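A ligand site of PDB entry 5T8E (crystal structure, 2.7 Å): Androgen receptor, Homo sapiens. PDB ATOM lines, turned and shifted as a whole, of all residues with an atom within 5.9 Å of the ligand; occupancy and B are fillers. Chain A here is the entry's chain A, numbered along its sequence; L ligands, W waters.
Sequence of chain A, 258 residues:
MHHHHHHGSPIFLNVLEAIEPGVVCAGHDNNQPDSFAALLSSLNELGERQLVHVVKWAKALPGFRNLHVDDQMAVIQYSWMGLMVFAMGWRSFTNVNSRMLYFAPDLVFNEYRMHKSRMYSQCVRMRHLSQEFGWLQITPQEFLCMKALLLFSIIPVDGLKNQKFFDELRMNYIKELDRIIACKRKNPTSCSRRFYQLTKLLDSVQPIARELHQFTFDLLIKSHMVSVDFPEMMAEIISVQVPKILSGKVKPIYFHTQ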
ATOM      1  N   LEU A  40      22.101  16.855 -12.005  1.00  0.00           N
ATOM      2  CA  LEU A  40      21.769  15.930 -10.921  1.00  0.00           C
ATOM      3  C   LEU A  40      20.488  15.133 -11.151  1.00  0.00           C
ATOM      4  O   LEU A  40      20.429  13.942 -10.819  1.00  0.00           O
ATOM      5  CB  LEU A  40      21.713  16.640  -9.562  1.00  0.00           C
ATOM      6  CG  LEU A  40      23.077  16.768  -8.845  1.00  0.00           C
ATOM      7  CD1 LEU A  40      23.552  15.420  -8.318  1.00  0.00           C
ATOM      8  CD2 LEU A  40      24.146  17.372  -9.746  1.00  0.00           C
ATOM      9  N   LEU A  43      21.606  12.358 -13.396  1.00  0.00           N
ATOM     10  CA  LEU A  43      22.326  11.346 -12.605  1.00  0.00           C
ATOM     11  C   LEU A  43      21.388  10.469 -11.774  1.00  0.00           C
ATOM     12  O   LEU A  43      21.547   9.263 -11.718  1.00  0.00           O
ATOM     13  CB  LEU A  43      23.363  11.997 -11.683  1.00  0.00           C
ATOM     14  CG  LEU A  43      24.696  12.439 -12.310  1.00  0.00           C
ATOM     15  CD1 LEU A  43      25.413  13.375 -11.355  1.00  0.00           C
ATOM     16  CD2 LEU A  43      25.609  11.263 -12.678  1.00  0.00           C
ATOM     17  N   ASN A  44      20.415  11.097 -11.113  1.00  0.00           N
ATOM     18  CA  ASN A  44      19.397  10.371 -10.327  1.00  0.00           C
ATOM     19  C   ASN A  44      18.548   9.404 -11.150  1.00  0.00           C
ATOM     20  O   ASN A  44      18.303   8.265 -10.744  1.00  0.00           O
ATOM     21  CB  ASN A  44      18.488  11.369  -9.585  1.00  0.00           C
ATOM     22  CG  ASN A  44      19.189  12.056  -8.427  1.00  0.00           C
ATOM     23  OD1 ASN A  44      20.296  11.682  -8.033  1.00  0.00           O
ATOM     24  ND2 ASN A  44      18.544  13.070  -7.863  1.00  0.00           N
ATOM     25  N   LEU A  46      19.574   8.111 -13.863  1.00  0.00           N
ATOM     26  CA  LEU A  46      20.551   7.102 -14.218  1.00  0.00           C
ATOM     27  C   LEU A  46      20.767   6.124 -13.050  1.00  0.00           C
ATOM     28  O   LEU A  46      20.841   4.913 -13.262  1.00  0.00           O
ATOM     29  CB  LEU A  46      21.880   7.748 -14.634  1.00  0.00           C
ATOM     30  CG  LEU A  46      23.072   6.802 -14.902  1.00  0.00           C
ATOM     31  CD1 LEU A  46      22.755   5.849 -16.054  1.00  0.00           C
ATOM     32  CD2 LEU A  46      24.331   7.578 -15.181  1.00  0.00           C
ATOM     33  N   GLY A  47      20.859   6.638 -11.837  1.00  0.00           N
ATOM     34  CA  GLY A  47      20.960   5.796 -10.647  1.00  0.00           C
ATOM     35  C   GLY A  47      19.788   4.831 -10.525  1.00  0.00           C
ATOM     36  O   GLY A  47      19.980   3.673 -10.164  1.00  0.00           O
ATOM     37  N   GLN A  50      20.398   2.253 -13.259  1.00  0.00           N
ATOM     38  CA  GLN A  50      21.509   1.400 -12.868  1.00  0.00           C
ATOM     39  C   GLN A  50      21.095   0.426 -11.772  1.00  0.00           C
ATOM     40  O   GLN A  50      21.535  -0.710 -11.746  1.00  0.00           O
ATOM     41  CB  GLN A  50      22.714   2.214 -12.371  1.00  0.00           C
ATOM     42  CG  GLN A  50      23.486   2.996 -13.426  1.00  0.00           C
ATOM     43  CD  GLN A  50      24.282   2.116 -14.389  1.00  0.00           C
ATOM     44  OE1 GLN A  50      24.106   0.902 -14.435  1.00  0.00           O
ATOM     45  NE2 GLN A  50      25.148   2.748 -15.169  1.00  0.00           N
ATOM     46  N   TRP A  80      24.898  -0.634  -3.614  1.00  0.00           N
ATOM     47  CA  TRP A  80      24.526  -0.028  -4.876  1.00  0.00           C
ATOM     48  C   TRP A  80      25.400   1.133  -5.321  1.00  0.00           C
ATOM     49  O   TRP A  80      25.793   1.198  -6.483  1.00  0.00           O
ATOM     50  CB  TRP A  80      23.057   0.391  -4.792  1.00  0.00           C
ATOM     51  CG  TRP A  80      22.597   1.339  -5.825  1.00  0.00           C
ATOM     52  CD1 TRP A  80      22.410   1.096  -7.152  1.00  0.00           C
ATOM     53  CD2 TRP A  80      22.238   2.709  -5.612  1.00  0.00           C
ATOM     54  NE1 TRP A  80      21.967   2.232  -7.797  1.00  0.00           N
ATOM     55  CE2 TRP A  80      21.851   3.238  -6.860  1.00  0.00           C
ATOM     56  CE3 TRP A  80      22.212   3.532  -4.489  1.00  0.00           C
ATOM     57  CZ2 TRP A  80      21.452   4.560  -7.016  1.00  0.00           C
ATOM     58  CZ3 TRP A  80      21.814   4.855  -4.645  1.00  0.00           C
ATOM     59  CH2 TRP A  80      21.440   5.352  -5.895  1.00  0.00           C
ATOM     60  N   MET A  81      25.708   2.064  -4.421  1.00  0.00           N
ATOM     61  CA  MET A  81      26.536   3.211  -4.784  1.00  0.00           C
ATOM     62  C   MET A  81      27.964   2.799  -5.189  1.00  0.00           C
ATOM     63  O   MET A  81      28.455   3.209  -6.243  1.00  0.00           O
ATOM     64  CB  MET A  81      26.604   4.246  -3.650  1.00  0.00           C
ATOM     65  CG  MET A  81      27.273   5.560  -4.048  1.00  0.00           C
ATOM     66  SD  MET A  81      26.403   6.522  -5.320  1.00  0.00           S
ATOM     67  CE  MET A  81      25.049   7.224  -4.357  1.00  0.00           C
ATOM     68  N   MET A  84      28.058   1.021  -8.469  1.00  0.00           N
ATOM     69  CA  MET A  84      27.914   2.011  -9.540  1.00  0.00           C
ATOM     70  C   MET A  84      29.240   2.719  -9.787  1.00  0.00           C
ATOM     71  O   MET A  84      29.720   2.763 -10.919  1.00  0.00           O
ATOM     72  CB  MET A  84      26.816   3.027  -9.225  1.00  0.00           C
ATOM     73  CG  MET A  84      25.417   2.579  -9.591  1.00  0.00           C
ATOM     74  SD  MET A  84      24.311   3.990  -9.708  1.00  0.00           S
ATOM     75  CE  MET A  84      24.595   4.750  -8.100  1.00  0.00           C
ATOM     76  N   VAL A  85      29.821   3.258  -8.712  1.00  0.00           N
ATOM     77  CA  VAL A  85      31.082   3.969  -8.798  1.00  0.00           C
ATOM     78  C   VAL A  85      32.170   3.112  -9.432  1.00  0.00           C
ATOM     79  O   VAL A  85      32.946   3.600 -10.252  1.00  0.00           O
ATOM     80  CB  VAL A  85      31.585   4.418  -7.408  1.00  0.00           C
ATOM     81  CG1 VAL A  85      33.017   4.920  -7.491  1.00  0.00           C
ATOM     82  CG2 VAL A  85      30.692   5.519  -6.855  1.00  0.00           C
ATOM     83  N   MET A  88      31.411   2.444 -13.137  1.00  0.00           N
ATOM     84  CA  MET A  88      31.500   3.726 -13.843  1.00  0.00           C
ATOM     85  C   MET A  88      32.968   4.069 -14.138  1.00  0.00           C
ATOM     86  O   MET A  88      33.271   4.556 -15.215  1.00  0.00           O
ATOM     87  CB  MET A  88      30.798   4.844 -13.058  1.00  0.00           C
ATOM     88  CG  MET A  88      30.690   6.156 -13.813  1.00  0.00           C
ATOM     89  SD  MET A  88      32.103   7.293 -13.616  1.00  0.00           S
ATOM     90  CE  MET A  88      32.048   7.663 -11.855  1.00  0.00           C
ATOM     91  N   ARG A  91      34.201   1.909 -17.138  1.00  0.00           N
ATOM     92  CA  ARG A  91      33.732   2.539 -18.366  1.00  0.00           C
ATOM     93  C   ARG A  91      34.604   3.755 -18.713  1.00  0.00           C
ATOM     94  O   ARG A  91      34.970   3.940 -19.865  1.00  0.00           O
ATOM     95  CB  ARG A  91      32.298   3.037 -18.208  1.00  0.00           C
ATOM     96  CG  ARG A  91      31.239   1.976 -18.090  1.00  0.00           C
ATOM     97  CD  ARG A  91      29.858   2.578 -18.333  1.00  0.00           C
ATOM     98  NE  ARG A  91      29.424   3.491 -17.278  1.00  0.00           N
ATOM     99  CZ  ARG A  91      28.883   3.101 -16.117  1.00  0.00           C
ATOM    100  NH1 ARG A  91      28.742   1.809 -15.835  1.00  0.00           N
ATOM    101  NH2 ARG A  91      28.500   3.999 -15.225  1.00  0.00           N
ATOM    102  N   PHE A 103      29.679   8.344 -17.094  1.00  0.00           N
ATOM    103  CA  PHE A 103      28.497   7.858 -16.400  1.00  0.00           C
ATOM    104  C   PHE A 103      27.629   7.076 -17.369  1.00  0.00           C
ATOM    105  O   PHE A 103      27.171   5.982 -17.047  1.00  0.00           O
ATOM    106  CB  PHE A 103      27.708   9.020 -15.793  1.00  0.00           C
ATOM    107  CG  PHE A 103      28.406   9.694 -14.650  1.00  0.00           C
ATOM    108  CD1 PHE A 103      28.526   9.049 -13.440  1.00  0.00           C
ATOM    109  CD2 PHE A 103      28.896  10.971 -14.775  1.00  0.00           C
ATOM    110  CE1 PHE A 103      29.152   9.658 -12.364  1.00  0.00           C
ATOM    111  CE2 PHE A 103      29.515  11.596 -13.698  1.00  0.00           C
ATOM    112  CZ  PHE A 103      29.642  10.936 -12.489  1.00  0.00           C
ATOM    113  N   ALA A 104      27.408   7.630 -18.557  1.00  0.00           N
ATOM    114  CA  ALA A 104      26.627   6.969 -19.596  1.00  0.00           C
ATOM    115  C   ALA A 104      27.007   7.541 -20.945  1.00  0.00           C
ATOM    116  O   ALA A 104      27.550   8.635 -21.007  1.00  0.00           O
ATOM    117  CB  ALA A 104      25.136   7.149 -19.344  1.00  0.00           C
ATOM    118  N   MET A 119      29.876  18.627  -7.526  1.00  0.00           N
ATOM    119  CA  MET A 119      30.411  17.370  -7.016  1.00  0.00           C
ATOM    120  C   MET A 119      31.894  17.240  -7.321  1.00  0.00           C
ATOM    121  O   MET A 119      32.422  16.120  -7.410  1.00  0.00           O
ATOM    122  CB  MET A 119      29.685  16.184  -7.655  1.00  0.00           C
ATOM    123  CG  MET A 119      28.364  15.804  -7.014  1.00  0.00           C
ATOM    124  SD  MET A 119      27.471  14.557  -7.994  1.00  0.00           S
ATOM    125  CE  MET A 119      28.779  13.408  -8.411  1.00  0.00           C
ATOM    126  N   MET A 126      36.563   9.923  -7.748  1.00  0.00           N
ATOM    127  CA  MET A 126      36.100   8.929  -8.718  1.00  0.00           C
ATOM    128  C   MET A 126      37.035   8.793  -9.910  1.00  0.00           C
ATOM    129  O   MET A 126      37.308   7.675 -10.352  1.00  0.00           O
ATOM    130  CB  MET A 126      34.679   9.254  -9.210  1.00  0.00           C
ATOM    131  CG  MET A 126      33.585   8.989  -8.178  1.00  0.00           C
ATOM    132  SD  MET A 126      31.901   9.151  -8.826  1.00  0.00           S
ATOM    133  CE  MET A 126      31.736  10.922  -8.935  1.00  0.00           C
ATOM    134  N   LEU A 212      29.769  10.102  -1.561  1.00  0.00           N
ATOM    135  CA  LEU A 212      28.628  10.195  -2.460  1.00  0.00           C
ATOM    136  C   LEU A 212      27.358   9.981  -1.702  1.00  0.00           C
ATOM    137  O   LEU A 212      26.344  10.632  -1.944  1.00  0.00           O
ATOM    138  CB  LEU A 212      28.739   9.143  -3.565  1.00  0.00           C
ATOM    139  CG  LEU A 212      29.695   9.518  -4.693  1.00  0.00           C
ATOM    140  CD1 LEU A 212      30.156   8.277  -5.436  1.00  0.00           C
ATOM    141  CD2 LEU A 212      29.037  10.511  -5.632  1.00  0.00           C
ATOM    142  N   PHE A 215      26.548  13.185   0.002  1.00  0.00           N
ATOM    143  CA  PHE A 215      26.169  14.249  -0.903  1.00  0.00           C
ATOM    144  C   PHE A 215      24.721  14.103  -1.348  1.00  0.00           C
ATOM    145  O   PHE A 215      23.940  15.073  -1.349  1.00  0.00           O
ATOM    146  CB  PHE A 215      27.090  14.243  -2.132  1.00  0.00           C
ATOM    147  CG  PHE A 215      26.727  15.272  -3.154  1.00  0.00           C
ATOM    148  CD1 PHE A 215      25.818  14.982  -4.163  1.00  0.00           C
ATOM    149  CD2 PHE A 215      27.285  16.560  -3.089  1.00  0.00           C
ATOM    150  CE1 PHE A 215      25.469  15.942  -5.105  1.00  0.00           C
ATOM    151  CE2 PHE A 215      26.938  17.526  -4.023  1.00  0.00           C
ATOM    152  CZ  PHE A 215      26.025  17.222  -5.035  1.00  0.00           C
ATOM    153  N   THR A 216      24.380  12.881  -1.765  1.00  0.00           N
ATOM    154  CA  THR A 216      23.040  12.556  -2.237  1.00  0.00           C
ATOM    155  C   THR A 216      22.012  12.676  -1.122  1.00  0.00           C
ATOM    156  O   THR A 216      20.864  13.070  -1.360  1.00  0.00           O
ATOM    157  CB  THR A 216      22.997  11.124  -2.810  1.00  0.00           C
ATOM    158  OG1 THR A 216      24.054  10.967  -3.770  1.00  0.00           O
ATOM    159  CG2 THR A 216      21.651  10.843  -3.483  1.00  0.00           C
ATOM    160  N   LEU A 219      21.527  16.269  -0.497  1.00  0.00           N
ATOM    161  CA  LEU A 219      20.824  16.766  -1.663  1.00  0.00           C
ATOM    162  C   LEU A 219      19.343  16.423  -1.624  1.00  0.00           C
ATOM    163  O   LEU A 219      18.499  17.239  -1.970  1.00  0.00           O
ATOM    164  CB  LEU A 219      21.453  16.177  -2.927  1.00  0.00           C
ATOM    165  CG  LEU A 219      20.879  16.630  -4.269  1.00  0.00           C
ATOM    166  CD1 LEU A 219      20.907  18.144  -4.379  1.00  0.00           C
ATOM    167  CD2 LEU A 219      21.665  15.979  -5.389  1.00  0.00           C
ATOM    168  N   PHE A 230      14.079  13.196  -7.587  1.00  0.00           N
ATOM    169  CA  PHE A 230      14.524  11.896  -7.107  1.00  0.00           C
ATOM    170  C   PHE A 230      13.477  10.824  -7.458  1.00  0.00           C
ATOM    171  O   PHE A 230      12.363  10.888  -6.957  1.00  0.00           O
ATOM    172  CB  PHE A 230      14.766  11.935  -5.598  1.00  0.00           C
ATOM    173  CG  PHE A 230      16.075  12.549  -5.200  1.00  0.00           C
ATOM    174  CD1 PHE A 230      16.237  13.932  -5.209  1.00  0.00           C
ATOM    175  CD2 PHE A 230      17.148  11.756  -4.826  1.00  0.00           C
ATOM    176  CE1 PHE A 230      17.447  14.506  -4.855  1.00  0.00           C
ATOM    177  CE2 PHE A 230      18.357  12.323  -4.466  1.00  0.00           C
ATOM    178  CZ  PHE A 230      18.506  13.694  -4.477  1.00  0.00           C
ATOM    179  N   MET A 234      15.019   5.061  -5.894  1.00  0.00           N
ATOM    180  CA  MET A 234      16.085   5.981  -5.514  1.00  0.00           C
ATOM    181  C   MET A 234      15.881   6.571  -4.116  1.00  0.00           C
ATOM    182  O   MET A 234      16.679   6.351  -3.210  1.00  0.00           O
ATOM    183  CB  MET A 234      16.102   7.117  -6.556  1.00  0.00           C
ATOM    184  CG  MET A 234      17.012   8.303  -6.279  1.00  0.00           C
ATOM    185  SD  MET A 234      18.714   8.023  -6.751  1.00  0.00           S
ATOM    186  CE  MET A 234      18.719   6.290  -7.243  1.00  0.00           C
ATOM    187  N   ILE A 238      17.768   6.174  -0.380  1.00  0.00           N
ATOM    188  CA  ILE A 238      18.510   7.282   0.216  1.00  0.00           C
ATOM    189  C   ILE A 238      17.958   7.715   1.568  1.00  0.00           C
ATOM    190  O   ILE A 238      18.728   8.100   2.430  1.00  0.00           O
ATOM    191  CB  ILE A 238      18.621   8.490  -0.730  1.00  0.00           C
ATOM    192  CG1 ILE A 238      19.457   8.117  -1.964  1.00  0.00           C
ATOM    193  CG2 ILE A 238      19.292   9.667  -0.039  1.00  0.00           C
ATOM    194  CD1 ILE A 238      19.028   8.842  -3.209  1.00  0.00           C
HETATM  195  C1  LIG L   1      23.510  11.382  -7.561  1.00  0.00           C
HETATM  196  C2  LIG L   1      24.976  11.704  -7.233  1.00  0.00           C
HETATM  197  C3  LIG L   1      25.736  10.797  -8.208  1.00  0.00           C
HETATM  198  C4  LIG L   1      25.288   8.669  -9.250  1.00  0.00           C
HETATM  199  C5  LIG L   1      25.901   6.938 -11.349  1.00  0.00           C
HETATM  200  C6  LIG L   1      22.764   8.942  -7.203  1.00  0.00           C
HETATM  201  C7  LIG L   1      23.512   9.923  -8.105  1.00  0.00           C
HETATM  202  O1  LIG L   1      22.696  11.555  -6.402  1.00  0.00           O
HETATM  203  N1  LIG L   1      24.954   9.524  -8.189  1.00  0.00           N
HETATM  204  C8  LIG L   1      24.332   8.355 -10.221  1.00  0.00           C
HETATM  205  C9  LIG L   1      24.624   7.499 -11.263  1.00  0.00           C
HETATM  206  C10 LIG L   1      26.220   6.058 -12.427  1.00  0.00           C
HETATM  207  N2  LIG L   1      26.369   5.368 -13.325  1.00  0.00           N
HETATM  208  C11 LIG L   1      26.876   7.248 -10.377  1.00  0.00           C
HETATM  209 CL1  LIG L   1      28.474   6.563 -10.459  1.00  0.00          CL
HETATM  210  C12 LIG L   1      26.572   8.098  -9.329  1.00  0.00           C
HETATM  211  C13 LIG L   1      27.644   8.384  -8.312  1.00  0.00           C
HETATM  212  O   HOH W   1      27.877   2.318 -13.289  1.00  0.00           O
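NH2 of Arg 91 lies within hydrogen-bond range of N2 of the ligand (3.2 Å).
A nitrogen (N2) of the ligand sits at hydrogen-bond distance from the side-chain amide nitrogen (NE2) of Gln 50, 3.4 Å away.
O1 of the ligand is in hydrogen-bond range of OD1 of Asn 44 (2.9 Å).
The side-chain hydroxyl of Thr 216 lies within hydrogen-bond range of an oxygen (O1) of the ligand, 3.0 Å away.
The guanidinium group of Arg 91 is in hydrogen-bond range of the backbone carbonyl oxygen of Phe 103 (3.0 Å).
The backbone carbonyl oxygen (O) of Gly 47 sits at hydrogen-bond distance from the indole nitrogen (NE1) of Trp 80.
O of Leu 212 is in hydrogen-bond range of OG1 of Thr 216.
The side-chain sulfur (SD) of Met 84 lies within hydrogen-bond range of the indole nitrogen (NE1) of Trp 80, at 3.5 Å.
Leu 43 touches the ligand.
Leu 46 touches the ligand.
Gly 47 touches the ligand (N to C9, 3.9 Å).
SD of Met 81 touches C13 of the ligand, 3.7 Å away.
Met 84 touches the ligand (SD to C5, 3.7 Å).
Val 85 touches the ligand (N to CL1, 3.97 Å).
Met 88 touches the ligand.
CE1 of Phe 103 touches CL1 of the ligand (3.7 Å).
Met 119 touches the ligand.
Leu 212 touches the ligand.
Hydrophobic or aromatic side chains within 4 Å of the ligand: Leu 46, Met 81, Met 84, Met 88, Phe 103, Met 119 and Leu 212.
14 residues have an atom within 4 Å of the ligand: Leu 43, Asn 44, Leu 46, Gly 47, Gln 50, Met 81, Met 84, Val 85, Met 88, Arg 91, Phe 103, Met 119, Leu 212 and Thr 216.
The nearest printed residue that does not touch the ligand is Trp 80 (4.04 Å).
Water W1 lies within hydrogen-bond range of NH2 of Arg 91, O of Met 84, NE2 of Gln 50 and N2 of the ligand.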
